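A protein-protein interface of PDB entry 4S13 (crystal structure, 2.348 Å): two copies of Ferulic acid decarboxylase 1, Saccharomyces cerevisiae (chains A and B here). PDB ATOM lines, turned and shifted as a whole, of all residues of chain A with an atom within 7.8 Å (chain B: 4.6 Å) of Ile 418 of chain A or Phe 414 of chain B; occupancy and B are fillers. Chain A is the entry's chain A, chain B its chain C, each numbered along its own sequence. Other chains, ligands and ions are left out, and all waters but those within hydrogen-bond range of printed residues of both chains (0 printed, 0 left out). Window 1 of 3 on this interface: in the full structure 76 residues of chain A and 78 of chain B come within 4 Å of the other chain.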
ATOM      1  N   PRO A 355     -30.413  -9.608  -1.509  1.00  0.00           N
ATOM      2  CA  PRO A 355     -29.992  -8.212  -1.266  1.00  0.00           C
ATOM      3  C   PRO A 355     -31.155  -7.288  -0.953  1.00  0.00           C
ATOM      4  O   PRO A 355     -32.139  -7.275  -1.687  1.00  0.00           O
ATOM      5  CB  PRO A 355     -29.335  -7.800  -2.589  1.00  0.00           C
ATOM      6  CG  PRO A 355     -28.838  -9.058  -3.148  1.00  0.00           C
ATOM      7  CD  PRO A 355     -29.839 -10.131  -2.754  1.00  0.00           C
ATOM      8  N   GLU A 357     -31.286  -4.037  -1.136  1.00  0.00           N
ATOM      9  CA  GLU A 357     -31.399  -3.016  -2.193  1.00  0.00           C
ATOM     10  C   GLU A 357     -32.294  -3.435  -3.354  1.00  0.00           C
ATOM     11  O   GLU A 357     -32.762  -2.590  -4.110  1.00  0.00           O
ATOM     12  CB  GLU A 357     -30.017  -2.663  -2.747  1.00  0.00           C
ATOM     13  CG  GLU A 357     -29.079  -1.992  -1.748  1.00  0.00           C
ATOM     14  CD  GLU A 357     -28.337  -2.958  -0.822  1.00  0.00           C
ATOM     15  OE1 GLU A 357     -28.736  -4.138  -0.701  1.00  0.00           O
ATOM     16  OE2 GLU A 357     -27.336  -2.516  -0.211  1.00  0.00           O
ATOM     17  N   TRP A 362     -34.636 -10.323  -5.692  1.00  0.00           N
ATOM     18  CA  TRP A 362     -33.458 -10.999  -6.216  1.00  0.00           C
ATOM     19  C   TRP A 362     -32.925 -12.062  -5.259  1.00  0.00           C
ATOM     20  O   TRP A 362     -32.592 -11.768  -4.129  1.00  0.00           O
ATOM     21  CB  TRP A 362     -32.320  -9.998  -6.495  1.00  0.00           C
ATOM     22  CG  TRP A 362     -32.429  -9.154  -7.724  1.00  0.00           C
ATOM     23  CD1 TRP A 362     -33.509  -9.017  -8.537  1.00  0.00           C
ATOM     24  CD2 TRP A 362     -31.395  -8.318  -8.281  1.00  0.00           C
ATOM     25  NE1 TRP A 362     -33.212  -8.157  -9.572  1.00  0.00           N
ATOM     26  CE2 TRP A 362     -31.924  -7.709  -9.430  1.00  0.00           C
ATOM     27  CE3 TRP A 362     -30.077  -8.021  -7.907  1.00  0.00           C
ATOM     28  CZ2 TRP A 362     -31.185  -6.815 -10.216  1.00  0.00           C
ATOM     29  CZ3 TRP A 362     -29.346  -7.145  -8.692  1.00  0.00           C
ATOM     30  CH2 TRP A 362     -29.900  -6.561  -9.840  1.00  0.00           C
ATOM     31  N   ILE A 364     -29.615 -14.262  -4.820  1.00  0.00           N
ATOM     32  CA  ILE A 364     -28.277 -14.448  -5.352  1.00  0.00           C
ATOM     33  C   ILE A 364     -27.701 -15.751  -4.820  1.00  0.00           C
ATOM     34  O   ILE A 364     -27.723 -15.989  -3.619  1.00  0.00           O
ATOM     35  CB  ILE A 364     -27.327 -13.294  -5.008  1.00  0.00           C
ATOM     36  CG1 ILE A 364     -27.542 -12.092  -5.934  1.00  0.00           C
ATOM     37  CG2 ILE A 364     -25.913 -13.710  -5.295  1.00  0.00           C
ATOM     38  CD1 ILE A 364     -28.846 -11.378  -5.832  1.00  0.00           C
ATOM     39  N   ILE A 403     -29.854 -14.913  -9.527  1.00  0.00           N
ATOM     40  CA  ILE A 403     -28.545 -14.574 -10.041  1.00  0.00           C
ATOM     41  C   ILE A 403     -27.436 -15.515  -9.574  1.00  0.00           C
ATOM     42  O   ILE A 403     -27.181 -15.642  -8.381  1.00  0.00           O
ATOM     43  CB  ILE A 403     -28.205 -13.128  -9.655  1.00  0.00           C
ATOM     44  CG1 ILE A 403     -29.265 -12.214 -10.266  1.00  0.00           C
ATOM     45  CG2 ILE A 403     -26.829 -12.740 -10.152  1.00  0.00           C
ATOM     46  CD1 ILE A 403     -29.284 -10.825  -9.726  1.00  0.00           C
ATOM     47  N   VAL A 405     -23.463 -16.478  -9.403  1.00  0.00           N
ATOM     48  CA  VAL A 405     -22.134 -15.866  -9.453  1.00  0.00           C
ATOM     49  C   VAL A 405     -21.090 -16.845  -8.969  1.00  0.00           C
ATOM     50  O   VAL A 405     -21.398 -17.770  -8.235  1.00  0.00           O
ATOM     51  CB  VAL A 405     -22.038 -14.581  -8.599  1.00  0.00           C
ATOM     52  CG1 VAL A 405     -22.804 -13.461  -9.230  1.00  0.00           C
ATOM     53  CG2 VAL A 405     -22.535 -14.837  -7.187  1.00  0.00           C
ATOM     54  N   ILE A 409     -17.272 -13.862  -5.299  1.00  0.00           N
ATOM     55  CA  ILE A 409     -18.160 -12.778  -4.932  1.00  0.00           C
ATOM     56  C   ILE A 409     -18.759 -12.988  -3.558  1.00  0.00           C
ATOM     57  O   ILE A 409     -19.485 -13.954  -3.328  1.00  0.00           O
ATOM     58  CB  ILE A 409     -19.305 -12.614  -5.943  1.00  0.00           C
ATOM     59  CG1 ILE A 409     -18.751 -12.286  -7.321  1.00  0.00           C
ATOM     60  CG2 ILE A 409     -20.248 -11.511  -5.505  1.00  0.00           C
ATOM     61  CD1 ILE A 409     -18.081 -10.950  -7.401  1.00  0.00           C
ATOM     62  N   ASP A 410     -18.448 -12.080  -2.643  1.00  0.00           N
ATOM     63  CA  ASP A 410     -19.127 -12.035  -1.360  1.00  0.00           C
ATOM     64  C   ASP A 410     -20.543 -11.516  -1.584  1.00  0.00           C
ATOM     65  O   ASP A 410     -20.755 -10.318  -1.730  1.00  0.00           O
ATOM     66  CB  ASP A 410     -18.352 -11.155  -0.376  1.00  0.00           C
ATOM     67  CG  ASP A 410     -19.114 -10.880   0.923  1.00  0.00           C
ATOM     68  OD1 ASP A 410     -20.118 -11.556   1.225  1.00  0.00           O
ATOM     69  OD2 ASP A 410     -18.680  -9.965   1.652  1.00  0.00           O
ATOM     70  N   ASN A 413     -22.404  -8.571   0.417  1.00  0.00           N
ATOM     71  CA  ASN A 413     -21.983  -7.185   0.151  1.00  0.00           C
ATOM     72  C   ASN A 413     -22.492  -6.720  -1.199  1.00  0.00           C
ATOM     73  O   ASN A 413     -21.991  -7.163  -2.222  1.00  0.00           O
ATOM     74  CB  ASN A 413     -20.457  -7.083   0.192  1.00  0.00           C
ATOM     75  CG  ASN A 413     -19.943  -5.681  -0.073  1.00  0.00           C
ATOM     76  OD1 ASN A 413     -20.704  -4.752  -0.359  1.00  0.00           O
ATOM     77  ND2 ASN A 413     -18.632  -5.518   0.052  1.00  0.00           N
ATOM     78  N   PHE A 414     -23.468  -5.824  -1.206  1.00  0.00           N
ATOM     79  CA  PHE A 414     -24.148  -5.491  -2.448  1.00  0.00           C
ATOM     80  C   PHE A 414     -23.248  -4.749  -3.445  1.00  0.00           C
ATOM     81  O   PHE A 414     -23.508  -4.769  -4.644  1.00  0.00           O
ATOM     82  CB  PHE A 414     -25.414  -4.675  -2.190  1.00  0.00           C
ATOM     83  CG  PHE A 414     -26.282  -4.524  -3.412  1.00  0.00           C
ATOM     84  CD1 PHE A 414     -26.969  -5.610  -3.920  1.00  0.00           C
ATOM     85  CD2 PHE A 414     -26.390  -3.301  -4.069  1.00  0.00           C
ATOM     86  CE1 PHE A 414     -27.764  -5.485  -5.062  1.00  0.00           C
ATOM     87  CE2 PHE A 414     -27.183  -3.167  -5.223  1.00  0.00           C
ATOM     88  CZ  PHE A 414     -27.873  -4.254  -5.723  1.00  0.00           C
ATOM     89  N   LYS A 415     -22.170  -4.144  -2.970  1.00  0.00           N
ATOM     90  CA  LYS A 415     -21.205  -3.546  -3.897  1.00  0.00           C
ATOM     91  C   LYS A 415     -20.518  -4.600  -4.768  1.00  0.00           C
ATOM     92  O   LYS A 415     -20.095  -4.306  -5.870  1.00  0.00           O
ATOM     93  CB  LYS A 415     -20.159  -2.727  -3.136  1.00  0.00           C
ATOM     94  CG  LYS A 415     -20.726  -1.466  -2.496  1.00  0.00           C
ATOM     95  CD  LYS A 415     -19.849  -0.976  -1.363  1.00  0.00           C
ATOM     96  CE  LYS A 415     -18.442  -0.672  -1.836  1.00  0.00           C
ATOM     97  NZ  LYS A 415     -17.598  -0.111  -0.740  1.00  0.00           N
ATOM     98  N   GLU A 416     -20.419  -5.831  -4.281  1.00  0.00           N
ATOM     99  CA  GLU A 416     -19.788  -6.892  -5.059  1.00  0.00           C
ATOM    100  C   GLU A 416     -20.809  -7.528  -5.998  1.00  0.00           C
ATOM    101  O   GLU A 416     -20.484  -7.922  -7.117  1.00  0.00           O
ATOM    102  CB  GLU A 416     -19.164  -7.945  -4.146  1.00  0.00           C
ATOM    103  CG  GLU A 416     -17.942  -7.437  -3.368  1.00  0.00           C
ATOM    104  CD  GLU A 416     -17.019  -8.562  -2.881  1.00  0.00           C
ATOM    105  OE1 GLU A 416     -17.042  -9.666  -3.472  1.00  0.00           O
ATOM    106  OE2 GLU A 416     -16.260  -8.342  -1.910  1.00  0.00           O
ATOM    107  N   VAL A 417     -22.052  -7.581  -5.543  1.00  0.00           N
ATOM    108  CA  VAL A 417     -23.127  -8.176  -6.310  1.00  0.00           C
ATOM    109  C   VAL A 417     -23.443  -7.371  -7.577  1.00  0.00           C
ATOM    110  O   VAL A 417     -23.486  -7.930  -8.670  1.00  0.00           O
ATOM    111  CB  VAL A 417     -24.391  -8.339  -5.428  1.00  0.00           C
ATOM    112  CG1 VAL A 417     -25.598  -8.705  -6.248  1.00  0.00           C
ATOM    113  CG2 VAL A 417     -24.139  -9.407  -4.394  1.00  0.00           C
ATOM    114  N   ILE A 418     -23.657  -6.067  -7.437  1.00  0.00           N
ATOM    115  CA  ILE A 418     -24.013  -5.242  -8.593  1.00  0.00           C
ATOM    116  C   ILE A 418     -22.836  -5.139  -9.576  1.00  0.00           C
ATOM    117  O   ILE A 418     -23.035  -5.061 -10.774  1.00  0.00           O
ATOM    118  CB  ILE A 418     -24.490  -3.835  -8.178  1.00  0.00           C
ATOM    119  CG1 ILE A 418     -25.248  -3.201  -9.328  1.00  0.00           C
ATOM    120  CG2 ILE A 418     -23.344  -2.947  -7.687  1.00  0.00           C
ATOM    121  CD1 ILE A 418     -26.460  -3.981  -9.691  1.00  0.00           C
ATOM    122  N   TRP A 419     -21.611  -5.189  -9.062  1.00  0.00           N
ATOM    123  CA  TRP A 419     -20.438  -5.293  -9.922  1.00  0.00           C
ATOM    124  C   TRP A 419     -20.481  -6.576 -10.739  1.00  0.00           C
ATOM    125  O   TRP A 419     -20.304  -6.546 -11.949  1.00  0.00           O
ATOM    126  CB  TRP A 419     -19.152  -5.249  -9.111  1.00  0.00           C
ATOM    127  CG  TRP A 419     -17.919  -5.528  -9.912  1.00  0.00           C
ATOM    128  CD1 TRP A 419     -17.474  -4.827 -10.986  1.00  0.00           C
ATOM    129  CD2 TRP A 419     -16.953  -6.565  -9.688  1.00  0.00           C
ATOM    130  NE1 TRP A 419     -16.297  -5.360 -11.457  1.00  0.00           N
ATOM    131  CE2 TRP A 419     -15.956  -6.430 -10.676  1.00  0.00           C
ATOM    132  CE3 TRP A 419     -16.837  -7.602  -8.752  1.00  0.00           C
ATOM    133  CZ2 TRP A 419     -14.858  -7.286 -10.752  1.00  0.00           C
ATOM    134  CZ3 TRP A 419     -15.740  -8.456  -8.830  1.00  0.00           C
ATOM    135  CH2 TRP A 419     -14.771  -8.291  -9.819  1.00  0.00           C
ATOM    136  N   ALA A 420     -20.726  -7.703 -10.079  1.00  0.00           N
ATOM    137  CA  ALA A 420     -20.767  -8.965 -10.788  1.00  0.00           C
ATOM    138  C   ALA A 420     -21.907  -9.003 -11.795  1.00  0.00           C
ATOM    139  O   ALA A 420     -21.718  -9.420 -12.928  1.00  0.00           O
ATOM    140  CB  ALA A 420     -20.881 -10.137  -9.804  1.00  0.00           C
ATOM    141  N   TYR A 421     -23.084  -8.562 -11.374  1.00  0.00           N
ATOM    142  CA  TYR A 421     -24.272  -8.617 -12.218  1.00  0.00           C
ATOM    143  C   TYR A 421     -24.093  -7.868 -13.543  1.00  0.00           C
ATOM    144  O   TYR A 421     -24.424  -8.377 -14.613  1.00  0.00           O
ATOM    145  CB  TYR A 421     -25.452  -8.054 -11.445  1.00  0.00           C
ATOM    146  CG  TYR A 421     -26.767  -8.013 -12.177  1.00  0.00           C
ATOM    147  CD1 TYR A 421     -27.570  -9.135 -12.247  1.00  0.00           C
ATOM    148  CD2 TYR A 421     -27.217  -6.841 -12.782  1.00  0.00           C
ATOM    149  CE1 TYR A 421     -28.781  -9.103 -12.898  1.00  0.00           C
ATOM    150  CE2 TYR A 421     -28.425  -6.801 -13.434  1.00  0.00           C
ATOM    151  CZ  TYR A 421     -29.204  -7.939 -13.488  1.00  0.00           C
ATOM    152  OH  TYR A 421     -30.410  -7.915 -14.131  1.00  0.00           O
ATOM    153  N   VAL A 422     -23.549  -6.663 -13.450  1.00  0.00           N
ATOM    154  CA  VAL A 422     -23.415  -5.757 -14.573  1.00  0.00           C
ATOM    155  C   VAL A 422     -22.324  -6.200 -15.580  1.00  0.00           C
ATOM    156  O   VAL A 422     -22.507  -6.116 -16.800  1.00  0.00           O
ATOM    157  CB  VAL A 422     -23.126  -4.319 -14.041  1.00  0.00           C
ATOM    158  CG1 VAL A 422     -22.401  -3.512 -15.041  1.00  0.00           C
ATOM    159  CG2 VAL A 422     -24.416  -3.625 -13.635  1.00  0.00           C
ATOM    160  N   THR A 423     -21.215  -6.708 -15.058  1.00  0.00           N
ATOM    161  CA  THR A 423     -20.054  -7.023 -15.876  1.00  0.00           C
ATOM    162  C   THR A 423     -19.921  -8.486 -16.296  1.00  0.00           C
ATOM    163  O   THR A 423     -19.110  -8.815 -17.161  1.00  0.00           O
ATOM    164  CB  THR A 423     -18.763  -6.620 -15.145  1.00  0.00           C
ATOM    165  OG1 THR A 423     -18.591  -7.441 -13.980  1.00  0.00           O
ATOM    166  CG2 THR A 423     -18.832  -5.150 -14.752  1.00  0.00           C
ATOM    167  N   ARG A 424     -20.716  -9.368 -15.712  1.00  0.00           N
ATOM    168  CA  ARG A 424     -20.524 -10.781 -15.994  1.00  0.00           C
ATOM    169  C   ARG A 424     -21.716 -11.445 -16.671  1.00  0.00           C
ATOM    170  O   ARG A 424     -21.682 -12.637 -16.928  1.00  0.00           O
ATOM    171  CB  ARG A 424     -20.181 -11.538 -14.713  1.00  0.00           C
ATOM    172  CG  ARG A 424     -18.986 -10.987 -13.941  1.00  0.00           C
ATOM    173  CD  ARG A 424     -18.515 -11.988 -12.880  1.00  0.00           C
ATOM    174  NE  ARG A 424     -17.478 -11.421 -12.030  1.00  0.00           N
ATOM    175  CZ  ARG A 424     -16.871 -12.074 -11.049  1.00  0.00           C
ATOM    176  NH1 ARG A 424     -17.197 -13.329 -10.777  1.00  0.00           N
ATOM    177  NH2 ARG A 424     -15.940 -11.471 -10.333  1.00  0.00           N
ATOM    178  N   HIS A 425     -22.766 -10.695 -16.967  1.00  0.00           N
ATOM    179  CA  HIS A 425     -23.813 -11.243 -17.822  1.00  0.00           C
ATOM    180  C   HIS A 425     -24.157 -10.328 -19.019  1.00  0.00           C
ATOM    181  O   HIS A 425     -24.182  -9.094 -18.918  1.00  0.00           O
ATOM    182  CB  HIS A 425     -25.067 -11.539 -17.007  1.00  0.00           C
ATOM    183  CG  HIS A 425     -26.082 -10.446 -17.024  1.00  0.00           C
ATOM    184  ND1 HIS A 425     -26.072  -9.412 -16.122  1.00  0.00           N
ATOM    185  CD2 HIS A 425     -27.156 -10.243 -17.824  1.00  0.00           C
ATOM    186  CE1 HIS A 425     -27.085  -8.598 -16.380  1.00  0.00           C
ATOM    187  NE2 HIS A 425     -27.754  -9.078 -17.409  1.00  0.00           N
ATOM    188  N   CYS A 464     -24.320 -15.187 -14.253  1.00  0.00           N
ATOM    189  CA  CYS A 464     -23.228 -14.211 -14.160  1.00  0.00           C
ATOM    190  C   CYS A 464     -21.944 -14.955 -13.853  1.00  0.00           C
ATOM    191  O   CYS A 464     -21.082 -14.484 -13.123  1.00  0.00           O
ATOM    192  CB  CYS A 464     -23.504 -13.107 -13.095  1.00  0.00           C
ATOM    193  SG  CYS A 464     -24.980 -12.119 -13.339  1.00  0.00           S
ATOM    194  N   PRO B 355     -24.399   5.523 -14.075  1.00  0.00           N
ATOM    195  CA  PRO B 355     -24.091   5.227 -12.676  1.00  0.00           C
ATOM    196  C   PRO B 355     -22.707   4.615 -12.539  1.00  0.00           C
ATOM    197  O   PRO B 355     -22.338   3.747 -13.328  1.00  0.00           O
ATOM    198  CB  PRO B 355     -25.181   4.222 -12.273  1.00  0.00           C
ATOM    199  CG  PRO B 355     -26.274   4.439 -13.235  1.00  0.00           C
ATOM    200  CD  PRO B 355     -25.624   4.847 -14.520  1.00  0.00           C
ATOM    201  N   GLU B 357     -21.697   2.763 -10.187  1.00  0.00           N
ATOM    202  CA  GLU B 357     -21.812   1.384  -9.701  1.00  0.00           C
ATOM    203  C   GLU B 357     -21.981   0.376 -10.832  1.00  0.00           C
ATOM    204  O   GLU B 357     -21.764  -0.810 -10.634  1.00  0.00           O
ATOM    205  CB  GLU B 357     -22.978   1.266  -8.718  1.00  0.00           C
ATOM    206  CG  GLU B 357     -22.764   2.035  -7.425  1.00  0.00           C
ATOM    207  CD  GLU B 357     -23.154   3.513  -7.474  1.00  0.00           C
ATOM    208  OE1 GLU B 357     -23.390   4.093  -8.564  1.00  0.00           O
ATOM    209  OE2 GLU B 357     -23.230   4.107  -6.385  1.00  0.00           O
ATOM    210  N   TRP B 362     -24.110   1.039 -17.950  1.00  0.00           N
ATOM    211  CA  TRP B 362     -25.517   1.436 -17.921  1.00  0.00           C
ATOM    212  C   TRP B 362     -25.676   2.910 -18.249  1.00  0.00           C
ATOM    213  O   TRP B 362     -24.957   3.749 -17.711  1.00  0.00           O
ATOM    214  CB  TRP B 362     -26.145   1.187 -16.537  1.00  0.00           C
ATOM    215  CG  TRP B 362     -26.505  -0.212 -16.216  1.00  0.00           C
ATOM    216  CD1 TRP B 362     -26.246  -1.324 -16.969  1.00  0.00           C
ATOM    217  CD2 TRP B 362     -27.208  -0.670 -15.054  1.00  0.00           C
ATOM    218  NE1 TRP B 362     -26.740  -2.430 -16.354  1.00  0.00           N
ATOM    219  CE2 TRP B 362     -27.329  -2.065 -15.172  1.00  0.00           C
ATOM    220  CE3 TRP B 362     -27.736  -0.034 -13.924  1.00  0.00           C
ATOM    221  CZ2 TRP B 362     -27.971  -2.848 -14.195  1.00  0.00           C
ATOM    222  CZ3 TRP B 362     -28.367  -0.803 -12.964  1.00  0.00           C
ATOM    223  CH2 TRP B 362     -28.485  -2.196 -13.105  1.00  0.00           C
ATOM    224  N   PHE B 412     -29.304  10.371 -10.605  1.00  0.00           N
ATOM    225  CA  PHE B 412     -27.951  10.576 -10.111  1.00  0.00           C
ATOM    226  C   PHE B 412     -27.739   9.956  -8.728  1.00  0.00           C
ATOM    227  O   PHE B 412     -26.636   9.956  -8.199  1.00  0.00           O
ATOM    228  CB  PHE B 412     -27.635  12.069 -10.090  1.00  0.00           C
ATOM    229  CG  PHE B 412     -27.795  12.723 -11.428  1.00  0.00           C
ATOM    230  CD1 PHE B 412     -26.773  12.679 -12.361  1.00  0.00           C
ATOM    231  CD2 PHE B 412     -28.984  13.349 -11.769  1.00  0.00           C
ATOM    232  CE1 PHE B 412     -26.931  13.267 -13.593  1.00  0.00           C
ATOM    233  CE2 PHE B 412     -29.138  13.925 -13.001  1.00  0.00           C
ATOM    234  CZ  PHE B 412     -28.112  13.882 -13.909  1.00  0.00           C
ATOM    235  N   ASN B 413     -28.807   9.416  -8.158  1.00  0.00           N
ATOM    236  CA  ASN B 413     -28.736   8.715  -6.887  1.00  0.00           C
ATOM    237  C   ASN B 413     -28.980   7.237  -7.110  1.00  0.00           C
ATOM    238  O   ASN B 413     -30.099   6.835  -7.406  1.00  0.00           O
ATOM    239  CB  ASN B 413     -29.766   9.285  -5.910  1.00  0.00           C
ATOM    240  CG  ASN B 413     -29.744   8.604  -4.549  1.00  0.00           C
ATOM    241  OD1 ASN B 413     -29.102   7.579  -4.348  1.00  0.00           O
ATOM    242  ND2 ASN B 413     -30.465   9.183  -3.605  1.00  0.00           N
ATOM    243  N   PHE B 414     -27.947   6.423  -6.941  1.00  0.00           N
ATOM    244  CA  PHE B 414     -28.048   5.009  -7.324  1.00  0.00           C
ATOM    245  C   PHE B 414     -29.048   4.218  -6.478  1.00  0.00           C
ATOM    246  O   PHE B 414     -29.607   3.239  -6.946  1.00  0.00           O
ATOM    247  CB  PHE B 414     -26.674   4.346  -7.269  1.00  0.00           C
ATOM    248  CG  PHE B 414     -26.646   2.995  -7.896  1.00  0.00           C
ATOM    249  CD1 PHE B 414     -26.913   2.847  -9.247  1.00  0.00           C
ATOM    250  CD2 PHE B 414     -26.363   1.864  -7.135  1.00  0.00           C
ATOM    251  CE1 PHE B 414     -26.902   1.594  -9.838  1.00  0.00           C
ATOM    252  CE2 PHE B 414     -26.345   0.606  -7.718  1.00  0.00           C
ATOM    253  CZ  PHE B 414     -26.618   0.469  -9.070  1.00  0.00           C
ATOM    254  N   LYS B 415     -29.299   4.659  -5.248  1.00  0.00           N
ATOM    255  CA  LYS B 415     -30.344   4.041  -4.430  1.00  0.00           C
ATOM    256  C   LYS B 415     -31.700   4.046  -5.129  1.00  0.00           C
ATOM    257  O   LYS B 415     -32.449   3.076  -5.051  1.00  0.00           O
ATOM    258  CB  LYS B 415     -30.472   4.752  -3.086  1.00  0.00           C
ATOM    259  CG  LYS B 415     -29.285   4.573  -2.155  1.00  0.00           C
ATOM    260  CD  LYS B 415     -29.295   5.640  -1.072  1.00  0.00           C
ATOM    261  CE  LYS B 415     -29.465   5.040   0.304  1.00  0.00           C
ATOM    262  NZ  LYS B 415     -28.219   4.346   0.732  1.00  0.00           N
ATOM    263  N   GLU B 416     -32.013   5.149  -5.791  1.00  0.00           N
ATOM    264  CA  GLU B 416     -33.266   5.302  -6.517  1.00  0.00           C
ATOM    265  C   GLU B 416     -33.248   4.566  -7.848  1.00  0.00           C
ATOM    266  O   GLU B 416     -34.264   4.064  -8.301  1.00  0.00           O
ATOM    267  CB  GLU B 416     -33.575   6.789  -6.776  1.00  0.00           C
ATOM    268  CG  GLU B 416     -33.737   7.627  -5.522  1.00  0.00           C
ATOM    269  CD  GLU B 416     -34.553   8.883  -5.749  1.00  0.00           C
ATOM    270  OE1 GLU B 416     -35.415   8.878  -6.644  1.00  0.00           O
ATOM    271  OE2 GLU B 416     -34.341   9.875  -5.024  1.00  0.00           O
ATOM    272  N   VAL B 417     -32.095   4.541  -8.492  1.00  0.00           N
ATOM    273  CA  VAL B 417     -31.974   3.870  -9.768  1.00  0.00           C
ATOM    274  C   VAL B 417     -32.185   2.366  -9.579  1.00  0.00           C
ATOM    275  O   VAL B 417     -33.014   1.764 -10.263  1.00  0.00           O
ATOM    276  CB  VAL B 417     -30.608   4.143 -10.415  1.00  0.00           C
ATOM    277  CG1 VAL B 417     -30.339   3.163 -11.532  1.00  0.00           C
ATOM    278  CG2 VAL B 417     -30.544   5.584 -10.902  1.00  0.00           C
ATOM    279  N   ILE B 418     -31.462   1.776  -8.629  1.00  0.00           N
ATOM    280  CA  ILE B 418     -31.574   0.349  -8.398  1.00  0.00           C
ATOM    281  C   ILE B 418     -32.989  -0.005  -7.925  1.00  0.00           C
ATOM    282  O   ILE B 418     -33.486  -1.059  -8.262  1.00  0.00           O
ATOM    283  CB  ILE B 418     -30.521  -0.159  -7.399  1.00  0.00           C
ATOM    284  CG1 ILE B 418     -30.378  -1.674  -7.501  1.00  0.00           C
ATOM    285  CG2 ILE B 418     -30.864   0.226  -5.967  1.00  0.00           C
ATOM    286  CD1 ILE B 418     -30.236  -2.197  -8.898  1.00  0.00           C
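Glu 357 of chain A touches Ile 418 of chain B (O to CG2, 3.9 Å).
Ile 418 of chain A touches Glu 357 of chain B.
Ile 418 of chain A touches Phe 414 of chain B (CG1 to CZ, 3.9 Å).
Trp 362 of chain B touches Val 422 of chain A.
Ile 418 of chain A touches just these residues of chain B: Glu 357 and Phe 414.
Phe 414 of chain B touches just one residue of chain A: Ile 418.
Of the printed residues of chain A, Trp 362 of chain B touches Val 422.
Of the printed residues of chain A, Glu 357 of chain B touches Ile 418.
Of the printed residues of chain A, Ile 418 of chain B touches Glu 357.
Of the printed residues of chain B, Val 422 of chain A touches Trp 362.
Of the printed residues of chain B, Glu 357 of chain A touches Ile 418 (3.9 Å).
Of the 22 printed residues of chain A, 3 touch a printed residue of chain B.
Hydrophobic or aromatic side chains of chain A within 4 Å of the printed part of chain B: Ile 418 and Val 422.
Of the 10 printed residues of chain B, 4 touch a printed residue of chain A.
Among the printed residues, no Asp or Glu carboxylate lies within 4 Å of a Lys or Arg side-chain nitrogen of the other chain.
Glu 357 of chain A touches Ile 418 of chain B, and with the chains exchanged Ile 418 of chain A touches Glu 357 of chain B.
Ile 418 of chain A touches Phe 414 of chain B, but with the chains exchanged Phe 414 of chain A does not touch Ile 418 of chain B (4.01 Å).
Of the 4 pairs that touch across the chains among the printed residues, 2 have their exchanged pair printed and touching as well.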
